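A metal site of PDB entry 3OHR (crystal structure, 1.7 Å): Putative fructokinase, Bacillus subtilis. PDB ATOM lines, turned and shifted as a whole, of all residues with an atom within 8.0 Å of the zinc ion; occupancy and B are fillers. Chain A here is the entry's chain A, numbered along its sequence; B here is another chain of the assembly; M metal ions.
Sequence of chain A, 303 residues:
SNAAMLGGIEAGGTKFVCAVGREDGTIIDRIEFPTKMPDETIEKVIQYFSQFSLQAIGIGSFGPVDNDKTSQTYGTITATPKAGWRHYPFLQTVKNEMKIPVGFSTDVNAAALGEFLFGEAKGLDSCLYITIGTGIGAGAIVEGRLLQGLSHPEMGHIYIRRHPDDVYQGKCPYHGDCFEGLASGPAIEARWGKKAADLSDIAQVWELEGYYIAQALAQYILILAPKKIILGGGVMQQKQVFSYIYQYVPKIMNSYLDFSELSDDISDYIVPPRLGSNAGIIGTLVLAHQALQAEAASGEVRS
OH of Tyr 159 lies within hydrogen-bond range of O of His 175 (2.7 Å). The backbone NH of Tyr 174 lies close to the side-chain sulfur of Cys 172. N of Gly 181 lies close to SG of Cys 178, at 3.4 Å. A ring nitrogen (NE2) of His 157 sits at hydrogen-bond distance from the side-chain hydroxyl (OH) of Tyr 256 of chain B (3.1 Å). The side-chain carboxylate of Glu 180 is in hydrogen-bond range of a ring nitrogen (NE2) of His 157, at 3.5 Å. A ring nitrogen (NE2) of His 175 sits at hydrogen-bond distance from the backbone carbonyl oxygen of Met 253 of chain B, at 3.1 Å.
Four residues have an atom within 4 Å of the zinc ion: His 157, Cys 172, His 175 and Cys 178. Along chain A the residues within 4 Å of the zinc ion span positions 157 to 178. The nearest printed residue that does not touch the zinc ion is Tyr 174 (4.6 Å).
The zinc ion is bound by ND1 of His 175 (2.0 Å). ND1 of His 157 binds the zinc ion (2.1 Å). The side-chain sulfur (SG) of Cys 178 is bound to the zinc ion (2.3 Å). The side-chain sulfur (SG) of Cys 172 binds the zinc ion, at 2.3 Å.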
ATOM      1  N   ILE A 136     -10.408 -24.081   0.892  1.00  0.00           N
ATOM      2  CA  ILE A 136      -9.812 -24.444  -0.355  1.00  0.00           C
ATOM      3  C   ILE A 136      -9.795 -23.220  -1.279  1.00  0.00           C
ATOM      4  O   ILE A 136     -10.803 -22.536  -1.424  1.00  0.00           O
ATOM      5  CB  ILE A 136     -10.495 -25.643  -1.054  1.00  0.00           C
ATOM      6  CG1 ILE A 136     -10.391 -26.902  -0.159  1.00  0.00           C
ATOM      7  CG2 ILE A 136      -9.811 -25.904  -2.413  1.00  0.00           C
ATOM      8  CD1 ILE A 136     -11.078 -28.131  -0.776  1.00  0.00           C
ATOM      9  N   GLU A 154     -12.316 -18.371  -7.271  1.00  0.00           N
ATOM     10  CA  GLU A 154     -12.729 -18.934  -5.987  1.00  0.00           C
ATOM     11  C   GLU A 154     -13.045 -20.404  -6.230  1.00  0.00           C
ATOM     12  O   GLU A 154     -14.174 -20.824  -6.071  1.00  0.00           O
ATOM     13  CB  GLU A 154     -13.874 -18.160  -5.395  1.00  0.00           C
ATOM     14  CG  GLU A 154     -13.376 -16.948  -4.588  1.00  0.00           C
ATOM     15  CD  GLU A 154     -12.661 -17.361  -3.318  1.00  0.00           C
ATOM     16  OE1 GLU A 154     -13.019 -18.398  -2.693  1.00  0.00           O
ATOM     17  OE2 GLU A 154     -11.724 -16.654  -2.929  1.00  0.00           O
ATOM     18  N   GLY A 156     -12.354 -23.097  -4.847  1.00  0.00           N
ATOM     19  CA  GLY A 156     -12.768 -23.980  -3.770  1.00  0.00           C
ATOM     20  C   GLY A 156     -14.244 -24.211  -3.623  1.00  0.00           C
ATOM     21  O   GLY A 156     -14.673 -25.146  -2.931  1.00  0.00           O
ATOM     22  N   HIS A 157     -15.042 -23.382  -4.267  1.00  0.00           N
ATOM     23  CA  HIS A 157     -16.483 -23.389  -4.034  1.00  0.00           C
ATOM     24  C   HIS A 157     -17.321 -23.982  -5.123  1.00  0.00           C
ATOM     25  O   HIS A 157     -18.464 -23.864  -5.151  1.00  0.00           O
ATOM     26  CB  HIS A 157     -16.993 -22.000  -3.602  1.00  0.00           C
ATOM     27  CG  HIS A 157     -16.417 -21.597  -2.290  1.00  0.00           C
ATOM     28  ND1 HIS A 157     -17.013 -21.876  -1.093  1.00  0.00           N
ATOM     29  CD2 HIS A 157     -15.244 -21.008  -1.986  1.00  0.00           C
ATOM     30  CE1 HIS A 157     -16.230 -21.513  -0.116  1.00  0.00           C
ATOM     31  NE2 HIS A 157     -15.156 -20.959  -0.636  1.00  0.00           N
ATOM     32  N   ILE A 158     -16.666 -24.650  -6.048  1.00  0.00           N
ATOM     33  CA  ILE A 158     -17.392 -25.371  -7.083  1.00  0.00           C
ATOM     34  C   ILE A 158     -18.117 -26.553  -6.481  1.00  0.00           C
ATOM     35  O   ILE A 158     -17.654 -27.217  -5.554  1.00  0.00           O
ATOM     36  CB  ILE A 158     -16.480 -25.837  -8.189  1.00  0.00           C
ATOM     37  CG1 ILE A 158     -15.382 -26.792  -7.699  1.00  0.00           C
ATOM     38  CG2 ILE A 158     -15.792 -24.638  -8.939  1.00  0.00           C
ATOM     39  CD1 ILE A 158     -14.705 -27.556  -8.851  1.00  0.00           C
ATOM     40  N   TYR A 159     -19.291 -26.877  -7.021  1.00  0.00           N
ATOM     41  CA  TYR A 159     -20.096 -28.044  -6.542  1.00  0.00           C
ATOM     42  C   TYR A 159     -19.845 -29.377  -7.322  1.00  0.00           C
ATOM     43  O   TYR A 159     -20.545 -29.657  -8.322  1.00  0.00           O
ATOM     44  CB  TYR A 159     -21.587 -27.710  -6.656  1.00  0.00           C
ATOM     45  CG  TYR A 159     -22.310 -26.965  -5.527  1.00  0.00           C
ATOM     46  CD1 TYR A 159     -22.934 -25.736  -5.767  1.00  0.00           C
ATOM     47  CD2 TYR A 159     -22.440 -27.497  -4.249  1.00  0.00           C
ATOM     48  CE1 TYR A 159     -23.619 -25.040  -4.792  1.00  0.00           C
ATOM     49  CE2 TYR A 159     -23.147 -26.824  -3.248  1.00  0.00           C
ATOM     50  CZ  TYR A 159     -23.761 -25.613  -3.530  1.00  0.00           C
ATOM     51  OH  TYR A 159     -24.471 -24.930  -2.552  1.00  0.00           O
ATOM     52  N   MLY A 171     -19.375 -28.455   5.225  1.00  0.00           N
ATOM     53  CA  MLY A 171     -18.868 -27.446   6.118  1.00  0.00           C
ATOM     54  CB  MLY A 171     -17.361 -27.748   6.320  1.00  0.00           C
ATOM     55  CG  MLY A 171     -16.721 -27.011   7.504  1.00  0.00           C
ATOM     56  CD  MLY A 171     -17.452 -27.168   8.856  1.00  0.00           C
ATOM     57  CE  MLY A 171     -16.593 -26.666   9.996  1.00  0.00           C
ATOM     58  NZ  MLY A 171     -17.417 -26.408  11.203  1.00  0.00           N
ATOM     59  CH1 MLY A 171     -17.784 -27.696  11.829  1.00  0.00           C
ATOM     60  CH2 MLY A 171     -16.661 -25.530  12.111  1.00  0.00           C
ATOM     61  C   MLY A 171     -19.069 -25.992   5.623  1.00  0.00           C
ATOM     62  O   MLY A 171     -19.026 -25.087   6.361  1.00  0.00           O
ATOM     63  N   CYS A 172     -19.277 -25.790   4.340  1.00  0.00           N
ATOM     64  CA  CYS A 172     -19.271 -24.424   3.823  1.00  0.00           C
ATOM     65  C   CYS A 172     -20.519 -23.645   4.238  1.00  0.00           C
ATOM     66  O   CYS A 172     -21.572 -24.082   3.978  1.00  0.00           O
ATOM     67  CB  CYS A 172     -19.158 -24.416   2.298  1.00  0.00           C
ATOM     68  SG  CYS A 172     -19.189 -22.734   1.628  1.00  0.00           S
ATOM     69  N   PRO A 173     -20.357 -22.494   4.881  1.00  0.00           N
ATOM     70  CA  PRO A 173     -21.509 -21.688   5.298  1.00  0.00           C
ATOM     71  C   PRO A 173     -22.333 -21.140   4.166  1.00  0.00           C
ATOM     72  O   PRO A 173     -23.478 -20.861   4.335  1.00  0.00           O
ATOM     73  CB  PRO A 173     -20.871 -20.534   6.049  1.00  0.00           C
ATOM     74  CG  PRO A 173     -19.674 -20.990   6.467  1.00  0.00           C
ATOM     75  CD  PRO A 173     -19.146 -21.918   5.411  1.00  0.00           C
ATOM     76  N   TYR A 174     -21.705 -20.954   3.012  1.00  0.00           N
ATOM     77  CA  TYR A 174     -22.436 -20.469   1.872  1.00  0.00           C
ATOM     78  C   TYR A 174     -23.134 -21.541   1.081  1.00  0.00           C
ATOM     79  O   TYR A 174     -24.282 -21.378   0.699  1.00  0.00           O
ATOM     80  CB  TYR A 174     -21.513 -19.735   0.903  1.00  0.00           C
ATOM     81  CG  TYR A 174     -21.119 -18.367   1.323  1.00  0.00           C
ATOM     82  CD1 TYR A 174     -19.971 -18.164   2.086  1.00  0.00           C
ATOM     83  CD2 TYR A 174     -21.863 -17.249   0.934  1.00  0.00           C
ATOM     84  CE1 TYR A 174     -19.561 -16.895   2.487  1.00  0.00           C
ATOM     85  CE2 TYR A 174     -21.466 -15.978   1.329  1.00  0.00           C
ATOM     86  CZ  TYR A 174     -20.338 -15.796   2.096  1.00  0.00           C
ATOM     87  OH  TYR A 174     -19.991 -14.492   2.406  1.00  0.00           O
ATOM     88  N   HIS A 175     -22.475 -22.660   0.835  1.00  0.00           N
ATOM     89  CA  HIS A 175     -22.955 -23.657  -0.112  1.00  0.00           C
ATOM     90  C   HIS A 175     -23.257 -25.037   0.475  1.00  0.00           C
ATOM     91  O   HIS A 175     -23.830 -25.850  -0.148  1.00  0.00           O
ATOM     92  CB  HIS A 175     -21.942 -23.863  -1.227  1.00  0.00           C
ATOM     93  CG  HIS A 175     -21.444 -22.598  -1.833  1.00  0.00           C
ATOM     94  ND1 HIS A 175     -20.149 -22.174  -1.700  1.00  0.00           N
ATOM     95  CD2 HIS A 175     -22.077 -21.646  -2.549  1.00  0.00           C
ATOM     96  CE1 HIS A 175     -20.007 -21.029  -2.298  1.00  0.00           C
ATOM     97  NE2 HIS A 175     -21.162 -20.676  -2.822  1.00  0.00           N
ATOM     98  N   GLY A 176     -22.817 -25.246   1.667  1.00  0.00           N
ATOM     99  CA  GLY A 176     -22.846 -26.576   2.304  1.00  0.00           C
ATOM    100  C   GLY A 176     -21.806 -27.515   1.718  1.00  0.00           C
ATOM    101  O   GLY A 176     -20.714 -27.618   2.227  1.00  0.00           O
ATOM    102  N   ASP A 177     -22.196 -28.222   0.660  1.00  0.00           N
ATOM    103  CA  ASP A 177     -21.361 -29.297   0.093  1.00  0.00           C
ATOM    104  C   ASP A 177     -20.708 -28.961  -1.244  1.00  0.00           C
ATOM    105  O   ASP A 177     -20.596 -29.783  -2.155  1.00  0.00           O
ATOM    106  CB  ASP A 177     -22.120 -30.628   0.072  1.00  0.00           C
ATOM    107  CG  ASP A 177     -23.373 -30.596  -0.737  1.00  0.00           C
ATOM    108  OD1 ASP A 177     -23.688 -29.576  -1.409  1.00  0.00           O
ATOM    109  OD2 ASP A 177     -24.068 -31.648  -0.751  1.00  0.00           O
ATOM    110  N   CYS A 178     -20.155 -27.758  -1.327  1.00  0.00           N
ATOM    111  CA  CYS A 178     -19.243 -27.422  -2.386  1.00  0.00           C
ATOM    112  C   CYS A 178     -17.942 -28.175  -2.094  1.00  0.00           C
ATOM    113  O   CYS A 178     -17.829 -28.823  -1.110  1.00  0.00           O
ATOM    114  CB  CYS A 178     -18.997 -25.930  -2.431  1.00  0.00           C
ATOM    115  SG  CYS A 178     -18.343 -25.300  -0.909  1.00  0.00           S
ATOM    116  N   PHE A 179     -16.984 -28.075  -3.003  1.00  0.00           N
ATOM    117  CA  PHE A 179     -15.669 -28.774  -2.825  1.00  0.00           C
ATOM    118  C   PHE A 179     -15.049 -28.481  -1.448  1.00  0.00           C
ATOM    119  O   PHE A 179     -14.670 -29.377  -0.688  1.00  0.00           O
ATOM    120  CB  PHE A 179     -14.759 -28.358  -3.994  1.00  0.00           C
ATOM    121  CG  PHE A 179     -13.359 -28.857  -3.953  1.00  0.00           C
ATOM    122  CD1 PHE A 179     -13.021 -30.101  -3.436  1.00  0.00           C
ATOM    123  CD2 PHE A 179     -12.368 -28.148  -4.611  1.00  0.00           C
ATOM    124  CE1 PHE A 179     -11.696 -30.565  -3.493  1.00  0.00           C
ATOM    125  CE2 PHE A 179     -11.054 -28.580  -4.656  1.00  0.00           C
ATOM    126  CZ  PHE A 179     -10.729 -29.749  -4.082  1.00  0.00           C
ATOM    127  N   GLU A 180     -14.929 -27.208  -1.100  1.00  0.00           N
ATOM    128  CA  GLU A 180     -14.449 -26.831   0.208  1.00  0.00           C
ATOM    129  C   GLU A 180     -15.286 -27.459   1.330  1.00  0.00           C
ATOM    130  O   GLU A 180     -14.750 -27.991   2.278  1.00  0.00           O
ATOM    131  CB  GLU A 180     -14.375 -25.310   0.361  1.00  0.00           C
ATOM    132  CG  GLU A 180     -13.878 -24.858   1.731  1.00  0.00           C
ATOM    133  CD  GLU A 180     -13.813 -23.359   1.879  1.00  0.00           C
ATOM    134  OE1 GLU A 180     -12.872 -22.771   1.282  1.00  0.00           O
ATOM    135  OE2 GLU A 180     -14.686 -22.819   2.595  1.00  0.00           O
ATOM    136  N   GLY A 181     -16.599 -27.431   1.162  1.00  0.00           N
ATOM    137  CA  GLY A 181     -17.502 -27.972   2.144  1.00  0.00           C
ATOM    138  C   GLY A 181     -17.330 -29.463   2.353  1.00  0.00           C
ATOM    139  O   GLY A 181     -17.609 -29.980   3.420  1.00  0.00           O
ATOM    140  N   LEU A 182     -16.880 -30.171   1.321  1.00  0.00           N
ATOM    141  CA  LEU A 182     -16.687 -31.615   1.416  1.00  0.00           C
ATOM    142  C   LEU A 182     -15.250 -32.042   1.752  1.00  0.00           C
ATOM    143  O   LEU A 182     -15.075 -33.165   2.270  1.00  0.00           O
ATOM    144  CB  LEU A 182     -17.104 -32.255   0.102  1.00  0.00           C
ATOM    145  CG  LEU A 182     -18.583 -32.286  -0.222  1.00  0.00           C
ATOM    146  CD1 LEU A 182     -18.845 -32.658  -1.686  1.00  0.00           C
ATOM    147  CD2 LEU A 182     -19.343 -33.255   0.673  1.00  0.00           C
ATOM    148  N   LEU B 222     -16.592 -19.275 -11.054  1.00  0.00           N
ATOM    149  CA  LEU B 222     -15.672 -19.512  -9.943  1.00  0.00           C
ATOM    150  C   LEU B 222     -14.228 -19.820 -10.342  1.00  0.00           C
ATOM    151  O   LEU B 222     -13.293 -19.520  -9.593  1.00  0.00           O
ATOM    152  CB  LEU B 222     -16.223 -20.596  -9.046  1.00  0.00           C
ATOM    153  CG  LEU B 222     -17.487 -20.224  -8.292  1.00  0.00           C
ATOM    154  CD1 LEU B 222     -18.170 -21.522  -7.716  1.00  0.00           C
ATOM    155  CD2 LEU B 222     -17.174 -19.179  -7.122  1.00  0.00           C
ATOM    156  N   ILE B 252     -27.387 -20.832  -6.898  1.00  0.00           N
ATOM    157  CA  ILE B 252     -26.260 -21.722  -6.746  1.00  0.00           C
ATOM    158  C   ILE B 252     -25.061 -21.027  -6.085  1.00  0.00           C
ATOM    159  O   ILE B 252     -24.346 -21.622  -5.274  1.00  0.00           O
ATOM    160  CB  ILE B 252     -25.879 -22.237  -8.165  1.00  0.00           C
ATOM    161  CG1 ILE B 252     -27.014 -23.093  -8.727  1.00  0.00           C
ATOM    162  CG2 ILE B 252     -24.550 -23.024  -8.164  1.00  0.00           C
ATOM    163  CD1 ILE B 252     -26.887 -23.413 -10.267  1.00  0.00           C
ATOM    164  N   MET B 253     -24.803 -19.787  -6.482  1.00  0.00           N
ATOM    165  CA  MET B 253     -23.674 -19.066  -5.932  1.00  0.00           C
ATOM    166  C   MET B 253     -23.947 -18.598  -4.518  1.00  0.00           C
ATOM    167  O   MET B 253     -23.039 -18.426  -3.738  1.00  0.00           O
ATOM    168  CB  MET B 253     -23.369 -17.875  -6.806  1.00  0.00           C
ATOM    169  CG  MET B 253     -23.139 -18.287  -8.201  1.00  0.00           C
ATOM    170  SD  MET B 253     -21.373 -18.679  -8.533  1.00  0.00           S
ATOM    171  CE  MET B 253     -21.313 -17.627 -10.162  1.00  0.00           C
ATOM    172  N   TYR B 256     -22.052 -15.527  -2.805  1.00  0.00           N
ATOM    173  CA  TYR B 256     -20.652 -15.662  -2.448  1.00  0.00           C
ATOM    174  C   TYR B 256     -19.709 -14.571  -3.030  1.00  0.00           C
ATOM    175  O   TYR B 256     -18.786 -14.100  -2.335  1.00  0.00           O
ATOM    176  CB  TYR B 256     -20.144 -17.066  -2.764  1.00  0.00           C
ATOM    177  CG  TYR B 256     -18.746 -17.299  -2.245  1.00  0.00           C
ATOM    178  CD1 TYR B 256     -18.426 -17.157  -0.897  1.00  0.00           C
ATOM    179  CD2 TYR B 256     -17.709 -17.576  -3.098  1.00  0.00           C
ATOM    180  CE1 TYR B 256     -17.132 -17.355  -0.416  1.00  0.00           C
ATOM    181  CE2 TYR B 256     -16.417 -17.776  -2.631  1.00  0.00           C
ATOM    182  CZ  TYR B 256     -16.116 -17.682  -1.318  1.00  0.00           C
ATOM    183  OH  TYR B 256     -14.868 -17.854  -0.786  1.00  0.00           O
HETATM  184 ZN    ZN M   1     -18.659 -23.031  -0.635  1.00  0.00          ZN
